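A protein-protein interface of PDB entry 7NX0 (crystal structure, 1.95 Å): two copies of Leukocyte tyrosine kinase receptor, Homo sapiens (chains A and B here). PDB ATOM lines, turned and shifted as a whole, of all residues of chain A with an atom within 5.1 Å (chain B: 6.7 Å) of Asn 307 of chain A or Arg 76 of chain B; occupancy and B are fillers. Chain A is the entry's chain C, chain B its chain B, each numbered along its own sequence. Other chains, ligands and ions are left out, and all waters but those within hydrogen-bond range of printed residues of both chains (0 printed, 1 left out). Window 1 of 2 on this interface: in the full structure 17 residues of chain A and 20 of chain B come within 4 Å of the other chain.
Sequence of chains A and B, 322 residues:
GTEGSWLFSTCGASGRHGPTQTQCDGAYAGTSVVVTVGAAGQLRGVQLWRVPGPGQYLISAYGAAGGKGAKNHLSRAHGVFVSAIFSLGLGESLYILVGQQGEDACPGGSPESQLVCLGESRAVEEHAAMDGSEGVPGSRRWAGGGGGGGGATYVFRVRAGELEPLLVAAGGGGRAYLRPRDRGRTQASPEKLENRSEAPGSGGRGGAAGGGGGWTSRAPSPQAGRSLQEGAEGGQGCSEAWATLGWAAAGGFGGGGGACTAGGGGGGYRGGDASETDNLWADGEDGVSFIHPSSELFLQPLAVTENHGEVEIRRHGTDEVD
OD1 of Asn 307 of chain A lies within hydrogen-bond range of NH1 of Arg 76 of chain B (3.1 Å).
OD1 of Asn 307 of chain A lies close to OE2 of Glu 306 of chain B, 3.3 Å away.
The side-chain amide nitrogen of Asn 307 of chain A sits at hydrogen-bond distance from the side-chain amide oxygen of Asn 307 of chain B, 3.2 Å away.
OE2 of Glu 306 of chain A sits close to OE1 of Glu 306 of chain B (3.5 Å).
The backbone carbonyl oxygen (O) of Asn 307 of chain A sits at hydrogen-bond distance from the backbone NH (N) of Ala 65 of chain A (2.9 Å).
NE of Arg 76 of chain A sits close to NE2 of Gln 101 of chain A (3.5 Å).
The side-chain amide oxygen (OE1) of Gln 101 of chain A sits at hydrogen-bond distance from the side-chain amide nitrogen (ND2) of Asn 307 of chain A, 3.1 Å away.
O of Asn 307 of chain B lies within hydrogen-bond range of N of Ala 65 of chain B, at 3.0 Å.
The side-chain carboxylate of Asp 104 of chain B is in salt-bridge range of the guanidinium group of Arg 76 of chain B.
The side-chain amide nitrogen (ND2) of Asn 307 of chain B is in hydrogen-bond range of the side-chain amide oxygen (OE1) of Gln 101 of chain B, 2.9 Å away.
Arg 76 of chain A touches Asn 307 of chain B (NH1 to OD1, 3.6 Å).
Asn 307 of chain A touches just these residues of chain B: Arg 76, Glu 306 and Asn 307.
Arg 76 of chain B touches one residue of chain A.
Of the printed residues of chain B, Arg 76 of chain A touches Asn 307.
Printed residues of chain A within 4 Å of Asn 307 of chain B: Arg 76 (3.6 Å) and Asn 307 (3.2 Å).
Gln 101 of chain B touches none of the printed residues of chain A.
Arg 76 of chain A touches Asn 307 of chain B, and with the chains exchanged Asn 307 of chain A touches Arg 76 of chain B.
Glu 306 of chain A touches its own counterpart, Glu 306 of chain B.
Asn 307 of chain A touches Glu 306 of chain B, but with the chains exchanged Glu 306 of chain A does not touch Asn 307 of chain B (4.4 Å).
Asn 307 of chain A touches its own counterpart, Asn 307 of chain B.
Positions printed for both chains: 65, 76, 101, 305, 306 and 307.
Of the 5 pairs that touch across the chains among the printed residues, 4 have their exchanged pair printed and touching as well.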
ATOM      1  N   GLY A  63       7.712 -12.968 -26.292  1.00  0.00           N
ATOM      2  CA  GLY A  63       8.392 -11.691 -26.238  1.00  0.00           C
ATOM      3  C   GLY A  63       8.708 -11.288 -24.811  1.00  0.00           C
ATOM      4  O   GLY A  63       8.237 -11.890 -23.858  1.00  0.00           O
ATOM      5  N   ALA A  64       9.527 -10.251 -24.667  1.00  0.00           N
ATOM      6  CA  ALA A  64       9.960  -9.826 -23.345  1.00  0.00           C
ATOM      7  C   ALA A  64       9.048  -8.739 -22.783  1.00  0.00           C
ATOM      8  O   ALA A  64       8.474  -7.929 -23.513  1.00  0.00           O
ATOM      9  CB  ALA A  64      11.396  -9.307 -23.367  1.00  0.00           C
ATOM     10  N   ALA A  65       8.996  -8.685 -21.461  1.00  0.00           N
ATOM     11  CA  ALA A  65       8.270  -7.631 -20.765  1.00  0.00           C
ATOM     12  C   ALA A  65       8.971  -6.280 -20.883  1.00  0.00           C
ATOM     13  O   ALA A  65      10.181  -6.179 -21.118  1.00  0.00           O
ATOM     14  CB  ALA A  65       8.118  -7.992 -19.289  1.00  0.00           C
ATOM     15  N   ARG A  76       4.989  -4.845 -14.729  1.00  0.00           N
ATOM     16  CA  ARG A  76       5.492  -4.673 -16.081  1.00  0.00           C
ATOM     17  C   ARG A  76       4.421  -5.055 -17.093  1.00  0.00           C
ATOM     18  O   ARG A  76       3.619  -5.955 -16.851  1.00  0.00           O
ATOM     19  CB  ARG A  76       6.707  -5.564 -16.303  1.00  0.00           C
ATOM     20  CG  ARG A  76       7.859  -5.262 -15.392  1.00  0.00           C
ATOM     21  CD  ARG A  76       9.078  -6.135 -15.648  1.00  0.00           C
ATOM     22  NE  ARG A  76      10.136  -5.699 -14.755  1.00  0.00           N
ATOM     23  CZ  ARG A  76      10.330  -6.198 -13.542  1.00  0.00           C
ATOM     24  NH1 ARG A  76       9.558  -7.183 -13.104  1.00  0.00           N
ATOM     25  NH2 ARG A  76      11.292  -5.721 -12.768  1.00  0.00           N
ATOM     26  N   GLN A 101      14.217  -8.103 -21.677  1.00  0.00           N
ATOM     27  CA  GLN A 101      13.302  -7.202 -20.982  1.00  0.00           C
ATOM     28  C   GLN A 101      13.724  -5.748 -21.185  1.00  0.00           C
ATOM     29  O   GLN A 101      14.910  -5.425 -21.269  1.00  0.00           O
ATOM     30  CB  GLN A 101      13.277  -7.559 -19.495  1.00  0.00           C
ATOM     31  CG  GLN A 101      12.261  -6.840 -18.637  1.00  0.00           C
ATOM     32  CD  GLN A 101      12.634  -6.890 -17.152  1.00  0.00           C
ATOM     33  OE1 GLN A 101      12.573  -7.945 -16.513  1.00  0.00           O
ATOM     34  NE2 GLN A 101      13.048  -5.753 -16.613  1.00  0.00           N
ATOM     35  N   THR A 305       4.529 -13.045 -20.341  1.00  0.00           N
ATOM     36  CA  THR A 305       5.952 -13.078 -19.982  1.00  0.00           C
ATOM     37  C   THR A 305       6.304 -11.985 -18.978  1.00  0.00           C
ATOM     38  O   THR A 305       6.068 -10.810 -19.247  1.00  0.00           O
ATOM     39  CB  THR A 305       6.822 -12.903 -21.222  1.00  0.00           C
ATOM     40  OG1 THR A 305       6.414 -13.824 -22.238  1.00  0.00           O
ATOM     41  CG2 THR A 305       8.291 -13.122 -20.880  1.00  0.00           C
ATOM     42  N   GLU A 306       6.955 -12.368 -17.863  1.00  0.00           N
ATOM     43  CA  GLU A 306       7.237 -11.448 -16.761  1.00  0.00           C
ATOM     44  C   GLU A 306       8.574 -10.701 -16.874  1.00  0.00           C
ATOM     45  O   GLU A 306       8.709  -9.605 -16.308  1.00  0.00           O
ATOM     46  CB  GLU A 306       7.221 -12.196 -15.417  1.00  0.00           C
ATOM     47  CG  GLU A 306       5.851 -12.689 -14.938  1.00  0.00           C
ATOM     48  CD  GLU A 306       5.892 -13.366 -13.566  1.00  0.00           C
ATOM     49  OE1 GLU A 306       6.301 -12.720 -12.574  1.00  0.00           O
ATOM     50  OE2 GLU A 306       5.498 -14.551 -13.477  1.00  0.00           O
ATOM     51  N   ASN A 307       9.550 -11.240 -17.609  1.00  0.00           N
ATOM     52  CA  ASN A 307      10.963 -10.833 -17.618  1.00  0.00           C
ATOM     53  C   ASN A 307      11.428 -11.002 -19.068  1.00  0.00           C
ATOM     54  O   ASN A 307      10.883 -10.337 -19.952  1.00  0.00           O
ATOM     55  CB  ASN A 307      11.838 -11.578 -16.599  1.00  0.00           C
ATOM     56  CG  ASN A 307      11.620 -11.071 -15.143  1.00  0.00           C
ATOM     57  OD1 ASN A 307      12.148 -11.657 -14.196  1.00  0.00           O
ATOM     58  ND2 ASN A 307      10.845  -9.999 -14.966  1.00  0.00           N
ATOM     59  N   HIS A 308      12.574 -11.626 -19.285  1.00  0.00           N
ATOM     60  CA  HIS A 308      13.027 -11.921 -20.636  1.00  0.00           C
ATOM     61  C   HIS A 308      12.060 -12.857 -21.385  1.00  0.00           C
ATOM     62  O   HIS A 308      11.294 -13.633 -20.795  1.00  0.00           O
ATOM     63  CB  HIS A 308      14.408 -12.565 -20.601  1.00  0.00           C
ATOM     64  CG  HIS A 308      15.465 -11.694 -19.999  1.00  0.00           C
ATOM     65  ND1 HIS A 308      15.509 -10.343 -20.240  1.00  0.00           N
ATOM     66  CD2 HIS A 308      16.498 -11.963 -19.162  1.00  0.00           C
ATOM     67  CE1 HIS A 308      16.510  -9.807 -19.566  1.00  0.00           C
ATOM     68  NE2 HIS A 308      17.132 -10.770 -18.908  1.00  0.00           N
ATOM     69  N   GLY A 309      12.131 -12.789 -22.708  1.00  0.00           N
ATOM     70  CA  GLY A 309      11.435 -13.740 -23.546  1.00  0.00           C
ATOM     71  C   GLY A 309      12.125 -15.095 -23.562  1.00  0.00           C
ATOM     72  O   GLY A 309      13.080 -15.372 -22.833  1.00  0.00           O
ATOM     73  N   ALA B  65      12.023 -14.350  -4.818  1.00  0.00           N
ATOM     74  CA  ALA B  65      12.944 -15.236  -5.510  1.00  0.00           C
ATOM     75  C   ALA B  65      14.395 -14.897  -5.175  1.00  0.00           C
ATOM     76  O   ALA B  65      14.733 -13.776  -4.779  1.00  0.00           O
ATOM     77  CB  ALA B  65      12.739 -15.147  -7.030  1.00  0.00           C
ATOM     78  N   GLY B  66      15.261 -15.904  -5.336  1.00  0.00           N
ATOM     79  CA  GLY B  66      16.684 -15.688  -5.219  1.00  0.00           C
ATOM     80  C   GLY B  66      17.254 -15.104  -6.489  1.00  0.00           C
ATOM     81  O   GLY B  66      16.608 -15.075  -7.540  1.00  0.00           O
ATOM     82  N   GLY B  67      18.489 -14.627  -6.381  1.00  0.00           N
ATOM     83  CA  GLY B  67      19.169 -14.097  -7.537  1.00  0.00           C
ATOM     84  C   GLY B  67      19.810 -15.186  -8.387  1.00  0.00           C
ATOM     85  O   GLY B  67      20.009 -16.317  -7.955  1.00  0.00           O
ATOM     86  N   LYS B  68      20.119 -14.810  -9.617  1.00  0.00           N
ATOM     87  CA  LYS B  68      20.811 -15.668 -10.559  1.00  0.00           C
ATOM     88  C   LYS B  68      22.316 -15.488 -10.397  1.00  0.00           C
ATOM     89  O   LYS B  68      22.785 -14.448  -9.930  1.00  0.00           O
ATOM     90  CB  LYS B  68      20.390 -15.333 -11.989  1.00  0.00           C
ATOM     91  CG  LYS B  68      18.981 -15.788 -12.349  1.00  0.00           C
ATOM     92  CD  LYS B  68      18.598 -15.377 -13.767  1.00  0.00           C
ATOM     93  CE  LYS B  68      17.220 -15.922 -14.159  1.00  0.00           C
ATOM     94  NZ  LYS B  68      17.047 -15.991 -15.631  1.00  0.00           N
ATOM     95  N   HIS B  73      22.075 -19.236 -14.625  1.00  0.00           N
ATOM     96  CA  HIS B  73      21.033 -18.230 -14.814  1.00  0.00           C
ATOM     97  C   HIS B  73      19.828 -18.783 -15.570  1.00  0.00           C
ATOM     98  O   HIS B  73      18.995 -17.998 -16.050  1.00  0.00           O
ATOM     99  CB  HIS B  73      21.580 -16.993 -15.564  1.00  0.00           C
ATOM    100  CG  HIS B  73      22.335 -17.331 -16.810  1.00  0.00           C
ATOM    101  ND1 HIS B  73      21.736 -17.909 -17.910  1.00  0.00           N
ATOM    102  CD2 HIS B  73      23.646 -17.195 -17.126  1.00  0.00           C
ATOM    103  CE1 HIS B  73      22.642 -18.109 -18.848  1.00  0.00           C
ATOM    104  NE2 HIS B  73      23.809 -17.682 -18.401  1.00  0.00           N
ATOM    105  N   LEU B  74      19.704 -20.105 -15.674  1.00  0.00           N
ATOM    106  CA  LEU B  74      18.533 -20.691 -16.324  1.00  0.00           C
ATOM    107  C   LEU B  74      17.252 -20.259 -15.626  1.00  0.00           C
ATOM    108  O   LEU B  74      16.239 -19.975 -16.276  1.00  0.00           O
ATOM    109  CB  LEU B  74      18.640 -22.218 -16.319  1.00  0.00           C
ATOM    110  CG  LEU B  74      17.474 -23.045 -16.876  1.00  0.00           C
ATOM    111  CD1 LEU B  74      17.171 -22.599 -18.299  1.00  0.00           C
ATOM    112  CD2 LEU B  74      17.775 -24.542 -16.827  1.00  0.00           C
ATOM    113  N   SER B  75      17.279 -20.207 -14.301  1.00  0.00           N
ATOM    114  CA  SER B  75      16.100 -19.834 -13.541  1.00  0.00           C
ATOM    115  C   SER B  75      16.532 -19.414 -12.147  1.00  0.00           C
ATOM    116  O   SER B  75      17.650 -19.700 -11.708  1.00  0.00           O
ATOM    117  CB  SER B  75      15.106 -20.988 -13.460  1.00  0.00           C
ATOM    118  OG  SER B  75      15.728 -22.089 -12.832  1.00  0.00           O
ATOM    119  N   ARG B  76      15.637 -18.697 -11.486  1.00  0.00           N
ATOM    120  CA  ARG B  76      15.757 -18.353 -10.077  1.00  0.00           C
ATOM    121  C   ARG B  76      15.103 -19.438  -9.236  1.00  0.00           C
ATOM    122  O   ARG B  76      14.174 -20.114  -9.686  1.00  0.00           O
ATOM    123  CB  ARG B  76      15.058 -17.025  -9.788  1.00  0.00           C
ATOM    124  CG  ARG B  76      15.476 -15.903 -10.695  1.00  0.00           C
ATOM    125  CD  ARG B  76      14.864 -14.562 -10.303  1.00  0.00           C
ATOM    126  NE  ARG B  76      15.704 -13.522 -10.883  1.00  0.00           N
ATOM    127  CZ  ARG B  76      15.460 -12.951 -12.054  1.00  0.00           C
ATOM    128  NH1 ARG B  76      14.378 -13.292 -12.736  1.00  0.00           N
ATOM    129  NH2 ARG B  76      16.283 -12.036 -12.540  1.00  0.00           N
ATOM    130  N   ALA B  77      15.570 -19.586  -8.002  1.00  0.00           N
ATOM    131  CA  ALA B  77      14.779 -20.304  -7.011  1.00  0.00           C
ATOM    132  C   ALA B  77      13.607 -19.406  -6.621  1.00  0.00           C
ATOM    133  O   ALA B  77      13.815 -18.297  -6.125  1.00  0.00           O
ATOM    134  CB  ALA B  77      15.625 -20.669  -5.799  1.00  0.00           C
ATOM    135  N   HIS B  78      12.385 -19.848  -6.894  1.00  0.00           N
ATOM    136  CA  HIS B  78      11.226 -18.986  -6.722  1.00  0.00           C
ATOM    137  C   HIS B  78      10.817 -18.867  -5.260  1.00  0.00           C
ATOM    138  O   HIS B  78      10.912 -19.825  -4.487  1.00  0.00           O
ATOM    139  CB  HIS B  78      10.064 -19.522  -7.557  1.00  0.00           C
ATOM    140  CG  HIS B  78      10.392 -19.659  -9.013  1.00  0.00           C
ATOM    141  ND1 HIS B  78      10.250 -20.841  -9.706  1.00  0.00           N
ATOM    142  CD2 HIS B  78      10.845 -18.750  -9.909  1.00  0.00           C
ATOM    143  CE1 HIS B  78      10.608 -20.655 -10.966  1.00  0.00           C
ATOM    144  NE2 HIS B  78      10.969 -19.393 -11.115  1.00  0.00           N
ATOM    145  N   GLY B  79      10.378 -17.668  -4.883  1.00  0.00           N
ATOM    146  CA  GLY B  79       9.833 -17.471  -3.554  1.00  0.00           C
ATOM    147  C   GLY B  79       8.552 -18.259  -3.362  1.00  0.00           C
ATOM    148  O   GLY B  79       7.832 -18.571  -4.315  1.00  0.00           O
ATOM    149  N   GLN B 101      13.605  -9.375  -3.822  1.00  0.00           N
ATOM    150  CA  GLN B 101      14.389 -10.353  -4.562  1.00  0.00           C
ATOM    151  C   GLN B 101      15.862 -10.296  -4.174  1.00  0.00           C
ATOM    152  O   GLN B 101      16.430  -9.221  -3.966  1.00  0.00           O
ATOM    153  CB  GLN B 101      14.236 -10.095  -6.058  1.00  0.00           C
ATOM    154  CG  GLN B 101      14.780 -11.187  -6.951  1.00  0.00           C
ATOM    155  CD  GLN B 101      15.048 -10.695  -8.363  1.00  0.00           C
ATOM    156  OE1 GLN B 101      14.119 -10.424  -9.118  1.00  0.00           O
ATOM    157  NE2 GLN B 101      16.324 -10.555  -8.714  1.00  0.00           N
ATOM    158  N   GLY B 102      16.475 -11.472  -4.073  1.00  0.00           N
ATOM    159  CA  GLY B 102      17.923 -11.527  -4.006  1.00  0.00           C
ATOM    160  C   GLY B 102      18.526 -10.920  -5.260  1.00  0.00           C
ATOM    161  O   GLY B 102      18.009 -11.095  -6.364  1.00  0.00           O
ATOM    162  N   ASP B 104      20.630 -10.303  -8.485  1.00  0.00           N
ATOM    163  CA  ASP B 104      21.284 -11.105  -9.506  1.00  0.00           C
ATOM    164  C   ASP B 104      22.745 -10.704  -9.629  1.00  0.00           C
ATOM    165  O   ASP B 104      23.097  -9.535  -9.477  1.00  0.00           O
ATOM    166  CB  ASP B 104      20.602 -10.908 -10.858  1.00  0.00           C
ATOM    167  CG  ASP B 104      19.152 -11.358 -10.857  1.00  0.00           C
ATOM    168  OD1 ASP B 104      18.864 -12.439 -10.308  1.00  0.00           O
ATOM    169  OD2 ASP B 104      18.309 -10.636 -11.426  1.00  0.00           O
ATOM    170  N   CYS B 106      24.214 -10.593 -12.388  1.00  0.00           N
ATOM    171  CA  CYS B 106      24.287  -9.932 -13.681  1.00  0.00           C
ATOM    172  C   CYS B 106      22.978  -9.212 -13.945  1.00  0.00           C
ATOM    173  O   CYS B 106      21.919  -9.747 -13.622  1.00  0.00           O
ATOM    174  CB  CYS B 106      24.549 -10.955 -14.797  1.00  0.00           C
ATOM    175  SG  CYS B 106      26.065 -11.836 -14.515  1.00  0.00           S
ATOM    176  N   GLY B 173      16.762 -19.460  -2.292  1.00  0.00           N
ATOM    177  CA  GLY B 173      18.204 -19.327  -2.250  1.00  0.00           C
ATOM    178  C   GLY B 173      18.725 -18.737  -3.546  1.00  0.00           C
ATOM    179  O   GLY B 173      18.161 -18.935  -4.616  1.00  0.00           O
ATOM    180  N   ARG B 175      21.450 -18.347  -6.640  1.00  0.00           N
ATOM    181  CA  ARG B 175      22.224 -19.335  -7.377  1.00  0.00           C
ATOM    182  C   ARG B 175      23.715 -19.126  -7.162  1.00  0.00           C
ATOM    183  O   ARG B 175      24.195 -18.000  -7.027  1.00  0.00           O
ATOM    184  CB  ARG B 175      21.954 -19.269  -8.876  1.00  0.00           C
ATOM    185  CG  ARG B 175      20.503 -19.440  -9.253  1.00  0.00           C
ATOM    186  CD  ARG B 175      20.004 -20.800  -8.814  1.00  0.00           C
ATOM    187  NE  ARG B 175      18.771 -21.168  -9.507  1.00  0.00           N
ATOM    188  CZ  ARG B 175      17.953 -22.132  -9.105  1.00  0.00           C
ATOM    189  NH1 ARG B 175      18.238 -22.841  -8.024  1.00  0.00           N
ATOM    190  NH2 ARG B 175      16.846 -22.387  -9.794  1.00  0.00           N
ATOM    191  N   THR B 305       7.130 -17.533  -6.995  1.00  0.00           N
ATOM    192  CA  THR B 305       7.412 -16.132  -7.257  1.00  0.00           C
ATOM    193  C   THR B 305       8.685 -15.960  -8.080  1.00  0.00           C
ATOM    194  O   THR B 305       9.718 -16.552  -7.773  1.00  0.00           O
ATOM    195  CB  THR B 305       7.517 -15.400  -5.917  1.00  0.00           C
ATOM    196  OG1 THR B 305       6.259 -14.776  -5.619  1.00  0.00           O
ATOM    197  CG2 THR B 305       8.648 -14.411  -5.939  1.00  0.00           C
ATOM    198  N   GLU B 306       8.623 -15.099  -9.102  1.00  0.00           N
ATOM    199  CA  GLU B 306       9.758 -14.911 -10.006  1.00  0.00           C
ATOM    200  C   GLU B 306      10.655 -13.717  -9.652  1.00  0.00           C
ATOM    201  O   GLU B 306      11.808 -13.691 -10.077  1.00  0.00           O
ATOM    202  CB  GLU B 306       9.277 -14.753 -11.466  1.00  0.00           C
ATOM    203  CG  GLU B 306      10.173 -15.473 -12.501  1.00  0.00           C
ATOM    204  CD  GLU B 306       9.835 -15.169 -13.964  1.00  0.00           C
ATOM    205  OE1 GLU B 306       8.714 -15.495 -14.433  1.00  0.00           O
ATOM    206  OE2 GLU B 306      10.714 -14.607 -14.658  1.00  0.00           O
ATOM    207  N   ASN B 307      10.179 -12.772  -8.840  1.00  0.00           N
ATOM    208  CA  ASN B 307      10.781 -11.459  -8.591  1.00  0.00           C
ATOM    209  C   ASN B 307      10.466 -11.188  -7.116  1.00  0.00           C
ATOM    210  O   ASN B 307      10.849 -12.003  -6.275  1.00  0.00           O
ATOM    211  CB  ASN B 307      10.310 -10.390  -9.558  1.00  0.00           C
ATOM    212  CG  ASN B 307      10.838 -10.621 -10.967  1.00  0.00           C
ATOM    213  OD1 ASN B 307      10.096 -10.492 -11.927  1.00  0.00           O
ATOM    214  ND2 ASN B 307      12.118 -10.983 -11.094  1.00  0.00           N
